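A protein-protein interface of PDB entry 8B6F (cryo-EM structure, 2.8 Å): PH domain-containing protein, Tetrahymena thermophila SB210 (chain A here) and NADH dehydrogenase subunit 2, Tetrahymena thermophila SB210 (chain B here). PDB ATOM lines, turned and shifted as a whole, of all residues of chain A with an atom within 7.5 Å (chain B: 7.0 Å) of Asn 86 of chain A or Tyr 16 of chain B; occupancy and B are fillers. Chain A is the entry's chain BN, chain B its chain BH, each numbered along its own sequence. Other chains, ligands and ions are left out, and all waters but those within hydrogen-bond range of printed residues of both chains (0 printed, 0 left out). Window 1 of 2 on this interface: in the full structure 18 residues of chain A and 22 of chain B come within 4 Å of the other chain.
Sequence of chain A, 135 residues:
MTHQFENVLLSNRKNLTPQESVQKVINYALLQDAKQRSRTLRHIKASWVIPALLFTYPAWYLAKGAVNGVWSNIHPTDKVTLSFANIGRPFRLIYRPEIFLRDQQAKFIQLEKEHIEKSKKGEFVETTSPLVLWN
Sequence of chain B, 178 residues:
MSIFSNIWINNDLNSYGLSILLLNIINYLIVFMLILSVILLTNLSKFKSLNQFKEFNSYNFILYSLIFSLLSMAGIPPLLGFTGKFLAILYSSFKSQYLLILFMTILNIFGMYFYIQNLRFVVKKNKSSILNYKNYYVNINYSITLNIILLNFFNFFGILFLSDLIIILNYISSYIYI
The side-chain carboxylate (OD1) of Asp 12 of chain B is in salt-bridge range of the guanidinium group (NH1) of Arg 89 of chain A, 3.2 Å away.
O of Gly 88 of chain A sits at hydrogen-bond distance from N of Leu 13 of chain B (2.4 Å).
The side-chain hydroxyl (OH) of Tyr 16 of chain B sits at hydrogen-bond distance from the backbone carbonyl oxygen (O) of Asn 86 of chain A (3.3 Å).
The backbone carbonyl oxygen (O) of Ser 15 of chain B lies close to the side-chain amide oxygen (OD1) of Asn 170 of chain B (3.5 Å).
O of Tyr 16 of chain B is in hydrogen-bond range of OG of Ser 19 of chain B (2.5 Å).
The side-chain amide oxygen of Asn 170 of chain B sits at hydrogen-bond distance from the side-chain hydroxyl of Ser 19 of chain B (3.3 Å).
O of Asn 170 of chain B lies within hydrogen-bond range of OG of Ser 173 of chain B (3.1 Å).
O of Asn 170 of chain B lies close to OG of Ser 174 of chain B (3.5 Å).
O of Val 80 of chain A lies within hydrogen-bond range of OG of Ser 83 of chain A.
CD1 of Ile 166 of chain B touches CB of Ser 83 of chain A, 3.5 Å away.
Phe 84 of chain A touches Leu 87 of chain B (CD1 to CD2, 3.7 Å).
CD1 of Leu 90 of chain B touches O of Phe 84 of chain A, 3.8 Å away.
CD1 of Ile 87 of chain A touches OH of Tyr 16 of chain B, at 3.1 Å.
CD1 of Ile 87 of chain A touches CD2 of Leu 87 of chain B, 3.8 Å away.
Ile 87 of chain A touches Leu 90 of chain B (CD1 to CD1, 3.98 Å).
Gly 88 of chain A touches Asp 12 of chain B (O to C, 3.2 Å).
Tyr 16 of chain B touches Gly 88 of chain A.
Leu 13 of chain B touches Phe 91 of chain A.
Asn 170 of chain B touches Phe 91 of chain A.
Of chain B, only Tyr 16 comes within 4 Å of Asn 86 of chain A.
Tyr 16 of chain B touches just these residues of chain A: Asn 86, Ile 87 and Gly 88.
Of the printed residues of chain A, Leu 90 of chain B touches Phe 84 (3.8 Å) and Ile 87 (3.98 Å).
Of the printed residues of chain A, Leu 13 of chain B touches Gly 88 (2.4 Å) and Phe 91 (3.8 Å).
Printed residues of chain B within 4 Å of Arg 89 of chain A: Asp 12 and Phe 94.
The nearest residue of chain B that does not touch Asn 86 of chain A is Leu 87 of chain B (6.1 Å).
The nearest residue of chain A that does not touch Tyr 16 of chain B is Ser 83 of chain A (4.1 Å).
Of the 19 printed residues of chain B, 8 touch a printed residue of chain A.
Hydrophobic or aromatic side chains of chain B that line the printed part of chain A: Leu 13, Tyr 16, Leu 87, Leu 90, Phe 94 and Ile 166.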
ATOM      1  N   HIS A  75     -17.346 -20.309  16.223  1.00  0.00           N
ATOM      2  CA  HIS A  75     -17.723 -18.917  16.436  1.00  0.00           C
ATOM      3  C   HIS A  75     -16.498 -18.064  16.736  1.00  0.00           C
ATOM      4  O   HIS A  75     -15.597 -18.512  17.462  1.00  0.00           O
ATOM      5  CB  HIS A  75     -18.712 -18.806  17.596  1.00  0.00           C
ATOM      6  CG  HIS A  75     -19.538 -17.556  17.578  1.00  0.00           C
ATOM      7  ND1 HIS A  75     -19.176 -16.415  18.260  1.00  0.00           N
ATOM      8  CD2 HIS A  75     -20.711 -17.272  16.968  1.00  0.00           C
ATOM      9  CE1 HIS A  75     -20.087 -15.479  18.065  1.00  0.00           C
ATOM     10  NE2 HIS A  75     -21.030 -15.974  17.285  1.00  0.00           N
ATOM     11  N   THR A  77     -16.272 -15.525  18.725  1.00  0.00           N
ATOM     12  CA  THR A  77     -16.220 -15.267  20.157  1.00  0.00           C
ATOM     13  C   THR A  77     -15.762 -16.515  20.907  1.00  0.00           C
ATOM     14  O   THR A  77     -15.981 -17.646  20.471  1.00  0.00           O
ATOM     15  CB  THR A  77     -17.597 -14.823  20.661  1.00  0.00           C
ATOM     16  OG1 THR A  77     -18.016 -13.650  19.951  1.00  0.00           O
ATOM     17  CG2 THR A  77     -17.566 -14.514  22.147  1.00  0.00           C
ATOM     18  N   ASP A  78     -15.118 -16.297  22.050  1.00  0.00           N
ATOM     19  CA  ASP A  78     -14.618 -17.406  22.848  1.00  0.00           C
ATOM     20  C   ASP A  78     -15.773 -18.199  23.457  1.00  0.00           C
ATOM     21  O   ASP A  78     -16.899 -17.714  23.588  1.00  0.00           O
ATOM     22  CB  ASP A  78     -13.687 -16.906  23.952  1.00  0.00           C
ATOM     23  CG  ASP A  78     -14.295 -15.783  24.764  1.00  0.00           C
ATOM     24  OD1 ASP A  78     -14.955 -14.909  24.168  1.00  0.00           O
ATOM     25  OD2 ASP A  78     -14.113 -15.776  25.998  1.00  0.00           O
ATOM     26  N   VAL A  80     -16.317 -19.416  26.530  1.00  0.00           N
ATOM     27  CA  VAL A  80     -16.842 -18.972  27.819  1.00  0.00           C
ATOM     28  C   VAL A  80     -17.788 -17.795  27.628  1.00  0.00           C
ATOM     29  O   VAL A  80     -18.867 -17.739  28.229  1.00  0.00           O
ATOM     30  CB  VAL A  80     -15.689 -18.624  28.778  1.00  0.00           C
ATOM     31  CG1 VAL A  80     -16.231 -18.208  30.136  1.00  0.00           C
ATOM     32  CG2 VAL A  80     -14.745 -19.806  28.927  1.00  0.00           C
ATOM     33  N   THR A  81     -17.396 -16.835  26.791  1.00  0.00           N
ATOM     34  CA  THR A  81     -18.266 -15.701  26.501  1.00  0.00           C
ATOM     35  C   THR A  81     -19.550 -16.152  25.818  1.00  0.00           C
ATOM     36  O   THR A  81     -20.636 -15.653  26.129  1.00  0.00           O
ATOM     37  CB  THR A  81     -17.522 -14.693  25.630  1.00  0.00           C
ATOM     38  OG1 THR A  81     -16.307 -14.308  26.283  1.00  0.00           O
ATOM     39  CG2 THR A  81     -18.376 -13.458  25.379  1.00  0.00           C
ATOM     40  N   LEU A  82     -19.448 -17.101  24.888  1.00  0.00           N
ATOM     41  CA  LEU A  82     -20.645 -17.630  24.244  1.00  0.00           C
ATOM     42  C   LEU A  82     -21.585 -18.266  25.254  1.00  0.00           C
ATOM     43  O   LEU A  82     -22.803 -18.070  25.190  1.00  0.00           O
ATOM     44  CB  LEU A  82     -20.260 -18.656  23.184  1.00  0.00           C
ATOM     45  CG  LEU A  82     -19.811 -18.094  21.845  1.00  0.00           C
ATOM     46  CD1 LEU A  82     -19.274 -19.219  21.012  1.00  0.00           C
ATOM     47  CD2 LEU A  82     -20.954 -17.392  21.130  1.00  0.00           C
ATOM     48  N   SER A  83     -21.040 -19.034  26.194  1.00  0.00           N
ATOM     49  CA  SER A  83     -21.887 -19.736  27.147  1.00  0.00           C
ATOM     50  C   SER A  83     -22.607 -18.768  28.077  1.00  0.00           C
ATOM     51  O   SER A  83     -23.811 -18.911  28.315  1.00  0.00           O
ATOM     52  CB  SER A  83     -21.047 -20.731  27.949  1.00  0.00           C
ATOM     53  OG  SER A  83     -19.933 -20.094  28.547  1.00  0.00           O
ATOM     54  N   PHE A  84     -21.898 -17.770  28.603  1.00  0.00           N
ATOM     55  CA  PHE A  84     -22.445 -16.920  29.654  1.00  0.00           C
ATOM     56  C   PHE A  84     -23.035 -15.616  29.131  1.00  0.00           C
ATOM     57  O   PHE A  84     -24.148 -15.248  29.517  1.00  0.00           O
ATOM     58  CB  PHE A  84     -21.356 -16.613  30.686  1.00  0.00           C
ATOM     59  CG  PHE A  84     -20.945 -17.802  31.501  1.00  0.00           C
ATOM     60  CD1 PHE A  84     -21.795 -18.334  32.454  1.00  0.00           C
ATOM     61  CD2 PHE A  84     -19.699 -18.379  31.324  1.00  0.00           C
ATOM     62  CE1 PHE A  84     -21.414 -19.427  33.207  1.00  0.00           C
ATOM     63  CE2 PHE A  84     -19.312 -19.470  32.074  1.00  0.00           C
ATOM     64  CZ  PHE A  84     -20.170 -19.995  33.017  1.00  0.00           C
ATOM     65  N   ALA A  85     -22.315 -14.900  28.263  1.00  0.00           N
ATOM     66  CA  ALA A  85     -22.776 -13.577  27.847  1.00  0.00           C
ATOM     67  C   ALA A  85     -24.126 -13.648  27.143  1.00  0.00           C
ATOM     68  O   ALA A  85     -25.007 -12.818  27.394  1.00  0.00           O
ATOM     69  CB  ALA A  85     -21.738 -12.918  26.940  1.00  0.00           C
ATOM     70  N   ASN A  86     -24.307 -14.623  26.260  1.00  0.00           N
ATOM     71  CA  ASN A  86     -25.547 -14.752  25.502  1.00  0.00           C
ATOM     72  C   ASN A  86     -26.566 -15.516  26.338  1.00  0.00           C
ATOM     73  O   ASN A  86     -26.446 -16.731  26.518  1.00  0.00           O
ATOM     74  CB  ASN A  86     -25.285 -15.454  24.174  1.00  0.00           C
ATOM     75  CG  ASN A  86     -24.377 -14.653  23.268  1.00  0.00           C
ATOM     76  OD1 ASN A  86     -24.492 -13.431  23.181  1.00  0.00           O
ATOM     77  ND2 ASN A  86     -23.466 -15.335  22.589  1.00  0.00           N
ATOM     78  N   ILE A  87     -27.570 -14.808  26.849  1.00  0.00           N
ATOM     79  CA  ILE A  87     -28.617 -15.395  27.677  1.00  0.00           C
ATOM     80  C   ILE A  87     -29.952 -15.050  27.036  1.00  0.00           C
ATOM     81  O   ILE A  87     -30.332 -13.874  26.973  1.00  0.00           O
ATOM     82  CB  ILE A  87     -28.557 -14.890  29.126  1.00  0.00           C
ATOM     83  CG1 ILE A  87     -27.188 -15.184  29.747  1.00  0.00           C
ATOM     84  CG2 ILE A  87     -29.670 -15.514  29.960  1.00  0.00           C
ATOM     85  CD1 ILE A  87     -26.845 -16.655  29.845  1.00  0.00           C
ATOM     86  N   GLY A  88     -30.666 -16.068  26.560  1.00  0.00           N
ATOM     87  CA  GLY A  88     -31.993 -15.889  26.016  1.00  0.00           C
ATOM     88  C   GLY A  88     -32.052 -15.480  24.563  1.00  0.00           C
ATOM     89  O   GLY A  88     -33.135 -15.538  23.967  1.00  0.00           O
ATOM     90  N   ARG A  89     -30.943 -15.070  23.970  1.00  0.00           N
ATOM     91  CA  ARG A  89     -30.969 -14.642  22.583  1.00  0.00           C
ATOM     92  C   ARG A  89     -30.989 -15.849  21.644  1.00  0.00           C
ATOM     93  O   ARG A  89     -30.390 -16.885  21.942  1.00  0.00           O
ATOM     94  CB  ARG A  89     -29.755 -13.771  22.275  1.00  0.00           C
ATOM     95  CG  ARG A  89     -30.061 -12.282  22.223  1.00  0.00           C
ATOM     96  CD  ARG A  89     -30.782 -11.802  23.471  1.00  0.00           C
ATOM     97  NE  ARG A  89     -31.002 -10.362  23.443  1.00  0.00           N
ATOM     98  CZ  ARG A  89     -31.861  -9.721  24.224  1.00  0.00           C
ATOM     99  NH1 ARG A  89     -32.619 -10.366  25.093  1.00  0.00           N
ATOM    100  NH2 ARG A  89     -31.965  -8.400  24.126  1.00  0.00           N
ATOM    101  N   PRO A  90     -31.676 -15.743  20.507  1.00  0.00           N
ATOM    102  CA  PRO A  90     -31.718 -16.875  19.573  1.00  0.00           C
ATOM    103  C   PRO A  90     -30.332 -17.214  19.049  1.00  0.00           C
ATOM    104  O   PRO A  90     -29.513 -16.331  18.789  1.00  0.00           O
ATOM    105  CB  PRO A  90     -32.634 -16.379  18.448  1.00  0.00           C
ATOM    106  CG  PRO A  90     -33.426 -15.288  19.046  1.00  0.00           C
ATOM    107  CD  PRO A  90     -32.533 -14.636  20.050  1.00  0.00           C
ATOM    108  N   PHE A  91     -30.078 -18.512  18.888  1.00  0.00           N
ATOM    109  CA  PHE A  91     -28.846 -18.949  18.243  1.00  0.00           C
ATOM    110  C   PHE A  91     -28.787 -18.513  16.787  1.00  0.00           C
ATOM    111  O   PHE A  91     -27.692 -18.399  16.228  1.00  0.00           O
ATOM    112  CB  PHE A  91     -28.702 -20.464  18.352  1.00  0.00           C
ATOM    113  CG  PHE A  91     -28.391 -20.937  19.738  1.00  0.00           C
ATOM    114  CD1 PHE A  91     -29.385 -21.013  20.697  1.00  0.00           C
ATOM    115  CD2 PHE A  91     -27.102 -21.302  20.084  1.00  0.00           C
ATOM    116  CE1 PHE A  91     -29.101 -21.447  21.974  1.00  0.00           C
ATOM    117  CE2 PHE A  91     -26.810 -21.736  21.361  1.00  0.00           C
ATOM    118  CZ  PHE A  91     -27.811 -21.809  22.307  1.00  0.00           C
ATOM    119  N   LEU A  93     -29.553 -15.529  15.982  1.00  0.00           N
ATOM    120  CA  LEU A  93     -28.938 -14.215  16.122  1.00  0.00           C
ATOM    121  C   LEU A  93     -27.460 -14.326  16.480  1.00  0.00           C
ATOM    122  O   LEU A  93     -26.648 -13.518  16.021  1.00  0.00           O
ATOM    123  CB  LEU A  93     -29.686 -13.404  17.182  1.00  0.00           C
ATOM    124  CG  LEU A  93     -29.158 -12.001  17.488  1.00  0.00           C
ATOM    125  CD1 LEU A  93     -29.088 -11.157  16.228  1.00  0.00           C
ATOM    126  CD2 LEU A  93     -30.031 -11.329  18.533  1.00  0.00           C
ATOM    127  N   ILE A  94     -27.096 -15.309  17.305  1.00  0.00           N
ATOM    128  CA  ILE A  94     -25.696 -15.475  17.684  1.00  0.00           C
ATOM    129  C   ILE A  94     -24.869 -15.897  16.476  1.00  0.00           C
ATOM    130  O   ILE A  94     -23.816 -15.315  16.188  1.00  0.00           O
ATOM    131  CB  ILE A  94     -25.569 -16.486  18.838  1.00  0.00           C
ATOM    132  CG1 ILE A  94     -26.447 -16.072  20.023  1.00  0.00           C
ATOM    133  CG2 ILE A  94     -24.118 -16.606  19.287  1.00  0.00           C
ATOM    134  CD1 ILE A  94     -26.222 -14.658  20.515  1.00  0.00           C
ATOM    135  N   TYR A  95     -25.335 -16.910  15.750  1.00  0.00           N
ATOM    136  CA  TYR A  95     -24.683 -17.394  14.543  1.00  0.00           C
ATOM    137  C   TYR A  95     -25.531 -17.021  13.337  1.00  0.00           C
ATOM    138  O   TYR A  95     -26.755 -17.170  13.360  1.00  0.00           O
ATOM    139  CB  TYR A  95     -24.496 -18.915  14.571  1.00  0.00           C
ATOM    140  CG  TYR A  95     -23.846 -19.459  15.819  1.00  0.00           C
ATOM    141  CD1 TYR A  95     -24.554 -19.567  17.008  1.00  0.00           C
ATOM    142  CD2 TYR A  95     -22.534 -19.908  15.797  1.00  0.00           C
ATOM    143  CE1 TYR A  95     -23.966 -20.078  18.146  1.00  0.00           C
ATOM    144  CE2 TYR A  95     -21.936 -20.419  16.929  1.00  0.00           C
ATOM    145  CZ  TYR A  95     -22.656 -20.503  18.101  1.00  0.00           C
ATOM    146  OH  TYR A  95     -22.062 -21.016  19.228  1.00  0.00           O
ATOM    147  N   ASP B  12     -35.927 -13.041  22.012  1.00  0.00           N
ATOM    148  CA  ASP B  12     -35.864 -13.924  23.166  1.00  0.00           C
ATOM    149  C   ASP B  12     -36.128 -15.355  22.727  1.00  0.00           C
ATOM    150  O   ASP B  12     -37.034 -15.614  21.930  1.00  0.00           O
ATOM    151  CB  ASP B  12     -36.882 -13.514  24.234  1.00  0.00           C
ATOM    152  CG  ASP B  12     -36.680 -12.092  24.716  1.00  0.00           C
ATOM    153  OD1 ASP B  12     -35.526 -11.616  24.698  1.00  0.00           O
ATOM    154  OD2 ASP B  12     -37.673 -11.448  25.113  1.00  0.00           O
ATOM    155  N   LEU B  13     -35.329 -16.280  23.249  1.00  0.00           N
ATOM    156  CA  LEU B  13     -35.479 -17.704  22.978  1.00  0.00           C
ATOM    157  C   LEU B  13     -36.233 -18.320  24.149  1.00  0.00           C
ATOM    158  O   LEU B  13     -35.687 -18.447  25.250  1.00  0.00           O
ATOM    159  CB  LEU B  13     -34.117 -18.366  22.782  1.00  0.00           C
ATOM    160  CG  LEU B  13     -34.120 -19.847  22.397  1.00  0.00           C
ATOM    161  CD1 LEU B  13     -34.740 -20.046  21.025  1.00  0.00           C
ATOM    162  CD2 LEU B  13     -32.711 -20.406  22.436  1.00  0.00           C
ATOM    163  N   ASN B  14     -37.490 -18.700  23.913  1.00  0.00           N
ATOM    164  CA  ASN B  14     -38.330 -19.181  25.004  1.00  0.00           C
ATOM    165  C   ASN B  14     -37.791 -20.480  25.589  1.00  0.00           C
ATOM    166  O   ASN B  14     -37.839 -20.686  26.807  1.00  0.00           O
ATOM    167  CB  ASN B  14     -39.763 -19.371  24.509  1.00  0.00           C
ATOM    168  CG  ASN B  14     -40.754 -19.508  25.642  1.00  0.00           C
ATOM    169  OD1 ASN B  14     -40.389 -19.420  26.814  1.00  0.00           O
ATOM    170  ND2 ASN B  14     -42.018 -19.714  25.300  1.00  0.00           N
ATOM    171  N   SER B  15     -37.280 -21.367  24.739  1.00  0.00           N
ATOM    172  CA  SER B  15     -36.767 -22.663  25.182  1.00  0.00           C
ATOM    173  C   SER B  15     -35.314 -22.530  25.644  1.00  0.00           C
ATOM    174  O   SER B  15     -34.398 -23.162  25.119  1.00  0.00           O
ATOM    175  CB  SER B  15     -36.891 -23.680  24.057  1.00  0.00           C
ATOM    176  OG  SER B  15     -36.113 -23.274  22.944  1.00  0.00           O
ATOM    177  N   TYR B  16     -35.119 -21.689  26.649  1.00  0.00           N
ATOM    178  CA  TYR B  16     -33.807 -21.464  27.243  1.00  0.00           C
ATOM    179  C   TYR B  16     -33.781 -21.739  28.735  1.00  0.00           C
ATOM    180  O   TYR B  16     -32.791 -22.269  29.241  1.00  0.00           O
ATOM    181  CB  TYR B  16     -33.348 -20.022  26.981  1.00  0.00           C
ATOM    182  CG  TYR B  16     -31.897 -19.781  27.325  1.00  0.00           C
ATOM    183  CD1 TYR B  16     -31.524 -19.367  28.597  1.00  0.00           C
ATOM    184  CD2 TYR B  16     -30.900 -19.969  26.379  1.00  0.00           C
ATOM    185  CE1 TYR B  16     -30.199 -19.148  28.918  1.00  0.00           C
ATOM    186  CE2 TYR B  16     -29.572 -19.754  26.689  1.00  0.00           C
ATOM    187  CZ  TYR B  16     -29.228 -19.343  27.959  1.00  0.00           C
ATOM    188  OH  TYR B  16     -27.907 -19.128  28.272  1.00  0.00           O
ATOM    189  N   GLY B  17     -34.846 -21.391  29.455  1.00  0.00           N
ATOM    190  CA  GLY B  17     -34.909 -21.721  30.868  1.00  0.00           C
ATOM    191  C   GLY B  17     -34.909 -23.216  31.115  1.00  0.00           C
ATOM    192  O   GLY B  17     -34.272 -23.701  32.052  1.00  0.00           O
ATOM    193  N   LEU B  18     -35.623 -23.968  30.275  1.00  0.00           N
ATOM    194  CA  LEU B  18     -35.610 -25.423  30.388  1.00  0.00           C
ATOM    195  C   LEU B  18     -34.215 -25.981  30.143  1.00  0.00           C
ATOM    196  O   LEU B  18     -33.779 -26.907  30.834  1.00  0.00           O
ATOM    197  CB  LEU B  18     -36.613 -26.033  29.410  1.00  0.00           C
ATOM    198  CG  LEU B  18     -36.609 -27.562  29.299  1.00  0.00           C
ATOM    199  CD1 LEU B  18     -36.793 -28.219  30.657  1.00  0.00           C
ATOM    200  CD2 LEU B  18     -37.688 -28.021  28.337  1.00  0.00           C
ATOM    201  N   SER B  19     -33.500 -25.432  29.161  1.00  0.00           N
ATOM    202  CA  SER B  19     -32.133 -25.876  28.913  1.00  0.00           C
ATOM    203  C   SER B  19     -31.237 -25.586  30.110  1.00  0.00           C
ATOM    204  O   SER B  19     -30.382 -26.404  30.466  1.00  0.00           O
ATOM    205  CB  SER B  19     -31.583 -25.204  27.656  1.00  0.00           C
ATOM    206  OG  SER B  19     -31.379 -23.819  27.867  1.00  0.00           O
ATOM    207  N   ILE B  20     -31.410 -24.422  30.737  1.00  0.00           N
ATOM    208  CA  ILE B  20     -30.616 -24.091  31.917  1.00  0.00           C
ATOM    209  C   ILE B  20     -30.935 -25.051  33.056  1.00  0.00           C
ATOM    210  O   ILE B  20     -30.040 -25.487  33.788  1.00  0.00           O
ATOM    211  CB  ILE B  20     -30.848 -22.624  32.327  1.00  0.00           C
ATOM    212  CG1 ILE B  20     -30.314 -21.662  31.257  1.00  0.00           C
ATOM    213  CG2 ILE B  20     -30.192 -22.329  33.673  1.00  0.00           C
ATOM    214  CD1 ILE B  20     -28.839 -21.804  30.943  1.00  0.00           C
ATOM    215  N   LEU B  21     -32.215 -25.387  33.232  1.00  0.00           N
ATOM    216  CA  LEU B  21     -32.583 -26.340  34.272  1.00  0.00           C
ATOM    217  C   LEU B  21     -31.959 -27.704  34.007  1.00  0.00           C
ATOM    218  O   LEU B  21     -31.442 -28.348  34.926  1.00  0.00           O
ATOM    219  CB  LEU B  21     -34.104 -26.454  34.363  1.00  0.00           C
ATOM    220  CG  LEU B  21     -34.637 -27.408  35.434  1.00  0.00           C
ATOM    221  CD1 LEU B  21     -34.222 -26.960  36.825  1.00  0.00           C
ATOM    222  CD2 LEU B  21     -36.147 -27.512  35.334  1.00  0.00           C
ATOM    223  N   LEU B  22     -32.000 -28.162  32.755  1.00  0.00           N
ATOM    224  CA  LEU B  22     -31.355 -29.424  32.410  1.00  0.00           C
ATOM    225  C   LEU B  22     -29.857 -29.358  32.673  1.00  0.00           C
ATOM    226  O   LEU B  22     -29.261 -30.320  33.168  1.00  0.00           O
ATOM    227  CB  LEU B  22     -31.619 -29.774  30.946  1.00  0.00           C
ATOM    228  CG  LEU B  22     -33.057 -30.133  30.565  1.00  0.00           C
ATOM    229  CD1 LEU B  22     -33.157 -30.358  29.068  1.00  0.00           C
ATOM    230  CD2 LEU B  22     -33.540 -31.361  31.321  1.00  0.00           C
ATOM    231  N   LEU B  87     -25.436 -19.488  35.663  1.00  0.00           N
ATOM    232  CA  LEU B  87     -26.432 -19.434  34.600  1.00  0.00           C
ATOM    233  C   LEU B  87     -27.846 -19.326  35.152  1.00  0.00           C
ATOM    234  O   LEU B  87     -28.698 -18.675  34.538  1.00  0.00           O
ATOM    235  CB  LEU B  87     -26.293 -20.655  33.697  1.00  0.00           C
ATOM    236  CG  LEU B  87     -25.059 -20.631  32.794  1.00  0.00           C
ATOM    237  CD1 LEU B  87     -24.850 -21.974  32.133  1.00  0.00           C
ATOM    238  CD2 LEU B  87     -25.172 -19.539  31.742  1.00  0.00           C
ATOM    239  N   LEU B  90     -28.133 -15.742  35.984  1.00  0.00           N
ATOM    240  CA  LEU B  90     -28.240 -14.970  34.750  1.00  0.00           C
ATOM    241  C   LEU B  90     -29.645 -15.048  34.172  1.00  0.00           C
ATOM    242  O   LEU B  90     -30.194 -14.038  33.719  1.00  0.00           O
ATOM    243  CB  LEU B  90     -27.220 -15.471  33.728  1.00  0.00           C
ATOM    244  CG  LEU B  90     -25.786 -14.984  33.908  1.00  0.00           C
ATOM    245  CD1 LEU B  90     -24.814 -15.889  33.178  1.00  0.00           C
ATOM    246  CD2 LEU B  90     -25.663 -13.563  33.402  1.00  0.00           C
ATOM    247  N   TYR B  91     -30.240 -16.241  34.164  1.00  0.00           N
ATOM    248  CA  TYR B  91     -31.597 -16.374  33.651  1.00  0.00           C
ATOM    249  C   TYR B  91     -32.601 -15.662  34.549  1.00  0.00           C
ATOM    250  O   TYR B  91     -33.563 -15.061  34.058  1.00  0.00           O
ATOM    251  CB  TYR B  91     -31.960 -17.850  33.498  1.00  0.00           C
ATOM    252  CG  TYR B  91     -33.291 -18.065  32.821  1.00  0.00           C
ATOM    253  CD1 TYR B  91     -33.447 -17.831  31.463  1.00  0.00           C
ATOM    254  CD2 TYR B  91     -34.390 -18.506  33.540  1.00  0.00           C
ATOM    255  CE1 TYR B  91     -34.660 -18.025  30.841  1.00  0.00           C
ATOM    256  CE2 TYR B  91     -35.607 -18.703  32.930  1.00  0.00           C
ATOM    257  CZ  TYR B  91     -35.738 -18.463  31.580  1.00  0.00           C
ATOM    258  OH  TYR B  91     -36.951 -18.660  30.968  1.00  0.00           O
ATOM    259  N   PHE B  94     -32.372 -12.146  33.619  1.00  0.00           N
ATOM    260  CA  PHE B  94     -33.014 -11.963  32.323  1.00  0.00           C
ATOM    261  C   PHE B  94     -34.528 -11.908  32.468  1.00  0.00           C
ATOM    262  O   PHE B  94     -35.196 -11.110  31.799  1.00  0.00           O
ATOM    263  CB  PHE B  94     -32.599 -13.093  31.381  1.00  0.00           C
ATOM    264  CG  PHE B  94     -33.093 -12.927  29.976  1.00  0.00           C
ATOM    265  CD1 PHE B  94     -32.434 -12.091  29.096  1.00  0.00           C
ATOM    266  CD2 PHE B  94     -34.202 -13.623  29.529  1.00  0.00           C
ATOM    267  CE1 PHE B  94     -32.879 -11.939  27.802  1.00  0.00           C
ATOM    268  CE2 PHE B  94     -34.651 -13.476  28.235  1.00  0.00           C
ATOM    269  CZ  PHE B  94     -33.989 -12.632  27.369  1.00  0.00           C
ATOM    270  N   ILE B 166     -24.270 -26.342  26.253  1.00  0.00           N
ATOM    271  CA  ILE B 166     -25.413 -25.435  26.210  1.00  0.00           C
ATOM    272  C   ILE B 166     -26.101 -25.518  24.854  1.00  0.00           C
ATOM    273  O   ILE B 166     -27.335 -25.496  24.765  1.00  0.00           O
ATOM    274  CB  ILE B 166     -24.964 -23.999  26.540  1.00  0.00           C
ATOM    275  CG1 ILE B 166     -24.566 -23.909  28.016  1.00  0.00           C
ATOM    276  CG2 ILE B 166     -26.074 -22.996  26.223  1.00  0.00           C
ATOM    277  CD1 ILE B 166     -23.960 -22.586  28.413  1.00  0.00           C
ATOM    278  N   ASN B 170     -29.951 -26.702  24.493  1.00  0.00           N
ATOM    279  CA  ASN B 170     -30.917 -25.832  23.830  1.00  0.00           C
ATOM    280  C   ASN B 170     -31.517 -26.512  22.609  1.00  0.00           C
ATOM    281  O   ASN B 170     -32.705 -26.348  22.315  1.00  0.00           O
ATOM    282  CB  ASN B 170     -30.255 -24.514  23.437  1.00  0.00           C
ATOM    283  CG  ASN B 170     -30.135 -23.559  24.601  1.00  0.00           C
ATOM    284  OD1 ASN B 170     -30.977 -22.685  24.787  1.00  0.00           O
ATOM    285  ND2 ASN B 170     -29.086 -23.724  25.399  1.00  0.00           N
ATOM    286  N   SER B 173     -34.122 -28.889  23.945  1.00  0.00           N
ATOM    287  CA  SER B 173     -35.303 -28.228  24.489  1.00  0.00           C
ATOM    288  C   SER B 173     -36.107 -27.520  23.407  1.00  0.00           C
ATOM    289  O   SER B 173     -37.317 -27.331  23.567  1.00  0.00           O
ATOM    290  CB  SER B 173     -34.896 -27.238  25.580  1.00  0.00           C
ATOM    291  OG  SER B 173     -34.094 -26.197  25.053  1.00  0.00           O
ATOM    292  N   SER B 174     -35.469 -27.126  22.304  1.00  0.00           N
ATOM    293  CA  SER B 174     -36.186 -26.393  21.267  1.00  0.00           C
ATOM    294  C   SER B 174     -37.303 -27.221  20.654  1.00  0.00           C
ATOM    295  O   SER B 174     -38.251 -26.648  20.107  1.00  0.00           O
ATOM    296  CB  SER B 174     -35.220 -25.934  20.176  1.00  0.00           C
ATOM    297  OG  SER B 174     -34.620 -27.037  19.522  1.00  0.00           O
